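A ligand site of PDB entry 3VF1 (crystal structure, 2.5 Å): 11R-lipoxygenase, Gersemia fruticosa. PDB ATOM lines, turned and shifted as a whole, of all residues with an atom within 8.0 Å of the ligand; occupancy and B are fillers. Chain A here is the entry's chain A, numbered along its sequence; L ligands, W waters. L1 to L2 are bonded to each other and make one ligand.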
ATOM      1  N   ASP A 342      -6.515  35.790 -20.508  1.00  0.00           N
ATOM      2  CA  ASP A 342      -7.593  34.973 -19.938  1.00  0.00           C
ATOM      3  C   ASP A 342      -8.972  35.641 -19.947  1.00  0.00           C
ATOM      4  O   ASP A 342      -9.932  35.091 -19.402  1.00  0.00           O
ATOM      5  CB  ASP A 342      -7.237  34.515 -18.517  1.00  0.00           C
ATOM      6  CG  ASP A 342      -6.047  33.574 -18.483  1.00  0.00           C
ATOM      7  OD1 ASP A 342      -6.086  32.562 -19.222  1.00  0.00           O
ATOM      8  OD2 ASP A 342      -5.084  33.838 -17.740  1.00  0.00           O
ATOM      9  N   VAL A 476     -19.407  18.559 -12.372  1.00  0.00           N
ATOM     10  CA  VAL A 476     -18.038  18.267 -12.790  1.00  0.00           C
ATOM     11  C   VAL A 476     -17.978  17.828 -14.252  1.00  0.00           C
ATOM     12  O   VAL A 476     -17.139  18.318 -15.020  1.00  0.00           O
ATOM     13  CB  VAL A 476     -17.416  17.159 -11.911  1.00  0.00           C
ATOM     14  CG1 VAL A 476     -16.023  16.793 -12.431  1.00  0.00           C
ATOM     15  CG2 VAL A 476     -17.343  17.613 -10.464  1.00  0.00           C
ATOM     16  N   LEU A 479     -19.351  20.809 -16.897  1.00  0.00           N
ATOM     17  CA  LEU A 479     -18.336  21.804 -17.177  1.00  0.00           C
ATOM     18  C   LEU A 479     -17.224  21.208 -18.030  1.00  0.00           C
ATOM     19  O   LEU A 479     -16.635  21.895 -18.870  1.00  0.00           O
ATOM     20  CB  LEU A 479     -17.749  22.333 -15.871  1.00  0.00           C
ATOM     21  CG  LEU A 479     -18.688  23.132 -14.975  1.00  0.00           C
ATOM     22  CD1 LEU A 479     -18.021  23.447 -13.644  1.00  0.00           C
ATOM     23  CD2 LEU A 479     -19.116  24.417 -15.667  1.00  0.00           C
ATOM     24  N   ARG A 480     -16.943  19.929 -17.817  1.00  0.00           N
ATOM     25  CA  ARG A 480     -15.833  19.265 -18.504  1.00  0.00           C
ATOM     26  C   ARG A 480     -16.149  18.984 -19.965  1.00  0.00           C
ATOM     27  O   ARG A 480     -15.298  19.166 -20.840  1.00  0.00           O
ATOM     28  CB  ARG A 480     -15.476  17.966 -17.781  1.00  0.00           C
ATOM     29  CG  ARG A 480     -14.287  17.230 -18.378  1.00  0.00           C
ATOM     30  CD  ARG A 480     -13.977  15.982 -17.594  1.00  0.00           C
ATOM     31  NE  ARG A 480     -13.531  16.295 -16.235  1.00  0.00           N
ATOM     32  CZ  ARG A 480     -13.570  15.458 -15.203  1.00  0.00           C
ATOM     33  NH1 ARG A 480     -14.053  14.224 -15.361  1.00  0.00           N
ATOM     34  NH2 ARG A 480     -13.140  15.840 -14.012  1.00  0.00           N
ATOM     35  N   VAL A 484     -15.040  24.136 -20.548  1.00  0.00           N
ATOM     36  CA  VAL A 484     -14.934  25.460 -19.935  1.00  0.00           C
ATOM     37  C   VAL A 484     -14.387  25.398 -18.505  1.00  0.00           C
ATOM     38  O   VAL A 484     -14.240  26.423 -17.851  1.00  0.00           O
ATOM     39  CB  VAL A 484     -16.295  26.172 -19.895  1.00  0.00           C
ATOM     40  CG1 VAL A 484     -16.814  26.413 -21.310  1.00  0.00           C
ATOM     41  CG2 VAL A 484     -17.301  25.383 -19.063  1.00  0.00           C
ATOM     42  N   ASP A 485     -14.090  24.198 -18.024  1.00  0.00           N
ATOM     43  CA  ASP A 485     -13.668  24.025 -16.633  1.00  0.00           C
ATOM     44  C   ASP A 485     -12.223  24.471 -16.411  1.00  0.00           C
ATOM     45  O   ASP A 485     -11.767  24.542 -15.266  1.00  0.00           O
ATOM     46  CB  ASP A 485     -13.851  22.572 -16.196  1.00  0.00           C
ATOM     47  CG  ASP A 485     -12.990  21.604 -16.976  1.00  0.00           C
ATOM     48  OD1 ASP A 485     -12.512  21.976 -18.072  1.00  0.00           O
ATOM     49  OD2 ASP A 485     -12.787  20.473 -16.497  1.00  0.00           O
ATOM     50  N   GLY A 486     -11.501  24.778 -17.486  1.00  0.00           N
ATOM     51  CA  GLY A 486     -10.119  25.209 -17.386  1.00  0.00           C
ATOM     52  C   GLY A 486      -9.924  26.708 -17.435  1.00  0.00           C
ATOM     53  O   GLY A 486      -8.808  27.197 -17.256  1.00  0.00           O
ATOM     54  N   LEU A 487     -11.001  27.449 -17.688  1.00  0.00           N
ATOM     55  CA  LEU A 487     -10.920  28.905 -17.809  1.00  0.00           C
ATOM     56  C   LEU A 487     -10.530  29.569 -16.492  1.00  0.00           C
ATOM     57  O   LEU A 487     -11.191  29.401 -15.475  1.00  0.00           O
ATOM     58  CB  LEU A 487     -12.261  29.456 -18.298  1.00  0.00           C
ATOM     59  CG  LEU A 487     -12.672  29.024 -19.710  1.00  0.00           C
ATOM     60  CD1 LEU A 487     -14.036  29.600 -20.077  1.00  0.00           C
ATOM     61  CD2 LEU A 487     -11.633  29.448 -20.735  1.00  0.00           C
ATOM     62  N   ARG A 488      -9.431  30.324 -16.526  1.00  0.00           N
ATOM     63  CA  ARG A 488      -8.866  30.937 -15.333  1.00  0.00           C
ATOM     64  C   ARG A 488      -9.774  31.970 -14.673  1.00  0.00           C
ATOM     65  O   ARG A 488      -9.816  32.077 -13.444  1.00  0.00           O
ATOM     66  CB  ARG A 488      -7.522  31.593 -15.668  1.00  0.00           C
ATOM     67  CG  ARG A 488      -6.443  30.628 -16.116  1.00  0.00           C
ATOM     68  CD  ARG A 488      -5.812  29.905 -14.933  1.00  0.00           C
ATOM     69  NE  ARG A 488      -4.696  29.047 -15.345  1.00  0.00           N
ATOM     70  CZ  ARG A 488      -3.962  28.316 -14.515  1.00  0.00           C
ATOM     71  NH1 ARG A 488      -4.217  28.313 -13.213  1.00  0.00           N
ATOM     72  NH2 ARG A 488      -2.967  27.582 -14.992  1.00  0.00           N
ATOM     73  N   LYS A 489     -10.496  32.746 -15.484  1.00  0.00           N
ATOM     74  CA  LYS A 489     -11.321  33.834 -14.953  1.00  0.00           C
ATOM     75  C   LYS A 489     -12.813  33.493 -15.018  1.00  0.00           C
ATOM     76  O   LYS A 489     -13.649  34.370 -15.177  1.00  0.00           O
ATOM     77  CB  LYS A 489     -11.021  35.138 -15.711  1.00  0.00           C
ATOM     78  CG  LYS A 489      -9.535  35.508 -15.669  1.00  0.00           C
ATOM     79  CD  LYS A 489      -9.247  36.815 -16.385  1.00  0.00           C
ATOM     80  CE  LYS A 489      -9.479  38.010 -15.482  1.00  0.00           C
ATOM     81  NZ  LYS A 489      -8.984  39.271 -16.084  1.00  0.00           N
ATOM     82  N   PHE A 490     -13.111  32.203 -14.891  1.00  0.00           N
ATOM     83  CA  PHE A 490     -14.469  31.712 -14.801  1.00  0.00           C
ATOM     84  C   PHE A 490     -14.770  31.468 -13.316  1.00  0.00           C
ATOM     85  O   PHE A 490     -14.697  30.346 -12.827  1.00  0.00           O
ATOM     86  CB  PHE A 490     -14.602  30.411 -15.601  1.00  0.00           C
ATOM     87  CG  PHE A 490     -16.016  29.939 -15.813  1.00  0.00           C
ATOM     88  CD1 PHE A 490     -17.090  30.642 -15.294  1.00  0.00           C
ATOM     89  CD2 PHE A 490     -16.261  28.790 -16.536  1.00  0.00           C
ATOM     90  CE1 PHE A 490     -18.390  30.190 -15.510  1.00  0.00           C
ATOM     91  CE2 PHE A 490     -17.540  28.334 -16.740  1.00  0.00           C
ATOM     92  CZ  PHE A 490     -18.613  29.033 -16.235  1.00  0.00           C
ATOM     93  N   TYR A 491     -15.090  32.551 -12.609  1.00  0.00           N
ATOM     94  CA  TYR A 491     -15.161  32.515 -11.154  1.00  0.00           C
ATOM     95  C   TYR A 491     -16.304  31.655 -10.632  1.00  0.00           C
ATOM     96  O   TYR A 491     -16.174  31.006  -9.583  1.00  0.00           O
ATOM     97  CB  TYR A 491     -15.266  33.937 -10.604  1.00  0.00           C
ATOM     98  CG  TYR A 491     -14.117  34.817 -11.041  1.00  0.00           C
ATOM     99  CD1 TYR A 491     -12.813  34.339 -11.019  1.00  0.00           C
ATOM    100  CD2 TYR A 491     -14.330  36.109 -11.491  1.00  0.00           C
ATOM    101  CE1 TYR A 491     -11.747  35.124 -11.421  1.00  0.00           C
ATOM    102  CE2 TYR A 491     -13.281  36.909 -11.892  1.00  0.00           C
ATOM    103  CZ  TYR A 491     -11.993  36.406 -11.858  1.00  0.00           C
ATOM    104  OH  TYR A 491     -10.937  37.200 -12.263  1.00  0.00           O
ATOM    105  N   TYR A 492     -17.430  31.649 -11.334  1.00  0.00           N
ATOM    106  CA  TYR A 492     -18.533  30.771 -10.965  1.00  0.00           C
ATOM    107  C   TYR A 492     -18.066  29.316 -10.931  1.00  0.00           C
ATOM    108  O   TYR A 492     -18.411  28.569 -10.033  1.00  0.00           O
ATOM    109  CB  TYR A 492     -19.698  30.895 -11.944  1.00  0.00           C
ATOM    110  CG  TYR A 492     -20.598  29.678 -11.936  1.00  0.00           C
ATOM    111  CD1 TYR A 492     -20.340  28.604 -12.771  1.00  0.00           C
ATOM    112  CD2 TYR A 492     -21.686  29.596 -11.075  1.00  0.00           C
ATOM    113  CE1 TYR A 492     -21.146  27.479 -12.760  1.00  0.00           C
ATOM    114  CE2 TYR A 492     -22.504  28.483 -11.054  1.00  0.00           C
ATOM    115  CZ  TYR A 492     -22.224  27.428 -11.907  1.00  0.00           C
ATOM    116  OH  TYR A 492     -23.035  26.305 -11.904  1.00  0.00           O
ATOM    117  N   LYS A 493     -17.295  28.933 -11.932  1.00  0.00           N
ATOM    118  CA  LYS A 493     -16.837  27.554 -12.068  1.00  0.00           C
ATOM    119  C   LYS A 493     -15.918  27.163 -10.918  1.00  0.00           C
ATOM    120  O   LYS A 493     -16.060  26.082 -10.346  1.00  0.00           O
ATOM    121  CB  LYS A 493     -16.116  27.355 -13.406  1.00  0.00           C
ATOM    122  CG  LYS A 493     -15.390  26.035 -13.542  1.00  0.00           C
ATOM    123  CD  LYS A 493     -13.915  26.153 -13.175  1.00  0.00           C
ATOM    124  CE  LYS A 493     -13.170  27.058 -14.156  1.00  0.00           C
ATOM    125  NZ  LYS A 493     -11.710  27.138 -13.863  1.00  0.00           N
ATOM    126  N   ASP A 494     -14.982  28.037 -10.572  1.00  0.00           N
ATOM    127  CA  ASP A 494     -14.043  27.766  -9.489  1.00  0.00           C
ATOM    128  C   ASP A 494     -14.761  27.586  -8.159  1.00  0.00           C
ATOM    129  O   ASP A 494     -14.492  26.650  -7.413  1.00  0.00           O
ATOM    130  CB  ASP A 494     -13.005  28.879  -9.376  1.00  0.00           C
ATOM    131  CG  ASP A 494     -12.049  28.912 -10.544  1.00  0.00           C
ATOM    132  OD1 ASP A 494     -11.813  27.849 -11.157  1.00  0.00           O
ATOM    133  OD2 ASP A 494     -11.520  29.996 -10.857  1.00  0.00           O
ATOM    134  N   ASP A 495     -15.695  28.495  -7.869  1.00  0.00           N
ATOM    135  CA  ASP A 495     -16.399  28.482  -6.590  1.00  0.00           C
ATOM    136  C   ASP A 495     -17.409  27.346  -6.515  1.00  0.00           C
ATOM    137  O   ASP A 495     -17.533  26.677  -5.496  1.00  0.00           O
ATOM    138  CB  ASP A 495     -17.098  29.819  -6.358  1.00  0.00           C
ATOM    139  CG  ASP A 495     -16.130  30.986  -6.299  1.00  0.00           C
ATOM    140  OD1 ASP A 495     -14.938  30.757  -5.976  1.00  0.00           O
ATOM    141  OD2 ASP A 495     -16.546  32.133  -6.576  1.00  0.00           O
ATOM    142  N   ALA A 496     -18.148  27.129  -7.609  1.00  0.00           N
ATOM    143  CA  ALA A 496     -19.145  26.071  -7.656  1.00  0.00           C
ATOM    144  C   ALA A 496     -18.502  24.695  -7.479  1.00  0.00           C
ATOM    145  O   ALA A 496     -19.108  23.799  -6.887  1.00  0.00           O
ATOM    146  CB  ALA A 496     -19.902  26.132  -8.982  1.00  0.00           C
ATOM    147  N   LEU A 497     -17.285  24.527  -7.980  1.00  0.00           N
ATOM    148  CA  LEU A 497     -16.595  23.244  -7.902  1.00  0.00           C
ATOM    149  C   LEU A 497     -16.080  22.979  -6.481  1.00  0.00           C
ATOM    150  O   LEU A 497     -16.003  21.831  -6.060  1.00  0.00           O
ATOM    151  CB  LEU A 497     -15.450  23.173  -8.905  1.00  0.00           C
ATOM    152  CG  LEU A 497     -15.863  22.924 -10.366  1.00  0.00           C
ATOM    153  CD1 LEU A 497     -14.640  22.934 -11.269  1.00  0.00           C
ATOM    154  CD2 LEU A 497     -16.618  21.612 -10.504  1.00  0.00           C
ATOM    155  N   LEU A 498     -15.721  24.041  -5.770  1.00  0.00           N
ATOM    156  CA  LEU A 498     -15.316  23.897  -4.375  1.00  0.00           C
ATOM    157  C   LEU A 498     -16.508  23.476  -3.527  1.00  0.00           C
ATOM    158  O   LEU A 498     -16.399  22.589  -2.676  1.00  0.00           O
ATOM    159  CB  LEU A 498     -14.752  25.222  -3.839  1.00  0.00           C
ATOM    160  CG  LEU A 498     -13.404  25.681  -4.394  1.00  0.00           C
ATOM    161  CD1 LEU A 498     -13.033  27.035  -3.811  1.00  0.00           C
ATOM    162  CD2 LEU A 498     -12.323  24.659  -4.110  1.00  0.00           C
ATOM    163  N   ASN A 501     -17.779  19.786  -4.223  1.00  0.00           N
ATOM    164  CA  ASN A 501     -16.930  18.780  -3.577  1.00  0.00           C
ATOM    165  C   ASN A 501     -17.078  18.781  -2.061  1.00  0.00           C
ATOM    166  O   ASN A 501     -16.971  17.732  -1.418  1.00  0.00           O
ATOM    167  CB  ASN A 501     -15.474  18.994  -3.970  1.00  0.00           C
ATOM    168  CG  ASN A 501     -15.183  18.569  -5.404  1.00  0.00           C
ATOM    169  OD1 ASN A 501     -15.704  17.564  -5.879  1.00  0.00           O
ATOM    170  ND2 ASN A 501     -14.343  19.338  -6.090  1.00  0.00           N
ATOM    171  N   GLN A 672     -10.946  31.438   0.774  1.00  0.00           N
ATOM    172  CA  GLN A 672     -10.360  31.398  -0.567  1.00  0.00           C
ATOM    173  C   GLN A 672     -10.988  32.467  -1.465  1.00  0.00           C
ATOM    174  O   GLN A 672     -10.280  33.257  -2.080  1.00  0.00           O
ATOM    175  CB  GLN A 672     -10.570  30.027  -1.211  1.00  0.00           C
ATOM    176  CG  GLN A 672      -9.728  28.911  -0.617  1.00  0.00           C
ATOM    177  CD  GLN A 672      -9.811  27.633  -1.424  1.00  0.00           C
ATOM    178  OE1 GLN A 672      -9.655  27.654  -2.649  1.00  0.00           O
ATOM    179  NE2 GLN A 672     -10.060  26.513  -0.752  1.00  0.00           N
HETATM  180  C1  LIG L   1     -10.023  22.651 -13.223  1.00  0.00           C
HETATM  181  C2  LIG L   1     -10.355  21.189 -13.476  1.00  0.00           C
HETATM  182  C3  LIG L   1      -9.091  20.335 -13.418  1.00  0.00           C
HETATM  183  C4  LIG L   1      -8.043  20.910 -14.356  1.00  0.00           C
HETATM  184  C5  LIG L   1      -7.814  22.388 -14.070  1.00  0.00           C
HETATM  185  C6  LIG L   1      -6.835  22.973 -15.087  1.00  0.00           C
HETATM  186  O1  LIG L   1     -11.274  20.730 -12.521  1.00  0.00           O
HETATM  187  O2  LIG L   1      -9.389  19.000 -13.788  1.00  0.00           O
HETATM  188  O3  LIG L   1      -6.822  20.215 -14.207  1.00  0.00           O
HETATM  189  O4  LIG L   1      -9.040  23.098 -14.144  1.00  0.00           O
HETATM  190  O5  LIG L   1      -6.203  24.117 -14.545  1.00  0.00           O
HETATM  191  C1  LG2 L   2     -11.321  23.906 -10.712  1.00  0.00           C
HETATM  192  C2  LG2 L   2      -9.917  24.015 -11.306  1.00  0.00           C
HETATM  193  C3  LG2 L   2      -8.889  24.349 -10.240  1.00  0.00           C
HETATM  194  C4  LG2 L   2      -7.964  25.326 -10.919  1.00  0.00           C
HETATM  195  C5  LG2 L   2      -8.824  25.972 -11.988  1.00  0.00           C
HETATM  196  C6  LG2 L   2      -8.000  26.272 -13.231  1.00  0.00           C
HETATM  197  O1  LG2 L   2     -11.663  25.118 -10.094  1.00  0.00           O
HETATM  198  O2  LG2 L   2      -9.555  22.790 -11.902  1.00  0.00           O
HETATM  199  O3  LG2 L   2      -8.193  23.189  -9.817  1.00  0.00           O
HETATM  200  O4  LG2 L   2      -7.432  26.273 -10.028  1.00  0.00           O
HETATM  201  O5  LG2 L   2      -9.880  25.066 -12.262  1.00  0.00           O
HETATM  202  O6  LG2 L   2      -8.391  27.502 -13.807  1.00  0.00           O
HETATM  203  O   HOH W   1      -9.877  20.934  -9.345  1.00  0.00           O
HETATM  204  O   HOH W   2      -8.739  29.642 -11.992  1.00  0.00           O
HETATM  205  O   HOH W   3     -12.510  25.305  -7.751  1.00  0.00           O
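Water W3 lies within hydrogen-bond range of O of Asp 494 (2.4 Å) and O1 of LG2 L2 (2.5 Å). Water W2 lies within hydrogen-bond range of O6 of LG2 L2, OD2 of Asp 494 and O of Arg 488.
The side-chain carboxylate (OD1) of Asp 494 is in hydrogen-bond range of an oxygen (O1) of LG2 L2, at 2.9 Å. O6 of LG2 L2 sits at hydrogen-bond distance from O of Gly 486, 3.5 Å away. An oxygen (O5) of LG2 L2 sits at hydrogen-bond distance from the side-chain amino group of Lys 493 (3.2 Å).
NZ of Lys 493 lies within salt-bridge range of OD1 of Asp 494, 2.8 Å away. NZ of Lys 493 sits at hydrogen-bond distance from O of Leu 487 (2.8 Å). NZ of Lys 493 sits at hydrogen-bond distance from O of Asp 485, 3.0 Å away. The backbone carbonyl oxygen (O) of Leu 497 is in hydrogen-bond range of the side-chain amide nitrogen (ND2) of Asn 501, 3.0 Å away.
An oxygen (O4) of LIG L1 sits close to the backbone carbonyl oxygen (O) of Asp 485, at 3.3 Å. O of Leu 487 touches O6 of LG2 L2, 3.8 Å away. CD of Arg 488 touches O6 of LG2 L2, 3.7 Å away. CD1 of Leu 497 touches C1 of LG2 L2, 3.5 Å away. Hydrophobic or aromatic side chains that line the ligand: Leu 497. Within 4 Å of the ligand: Asp 485, Gly 486, Leu 487, Arg 488, Lys 493, Asp 494 and Leu 497. The nearest printed residue that does not touch the ligand is Arg 480 (4.9 Å).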
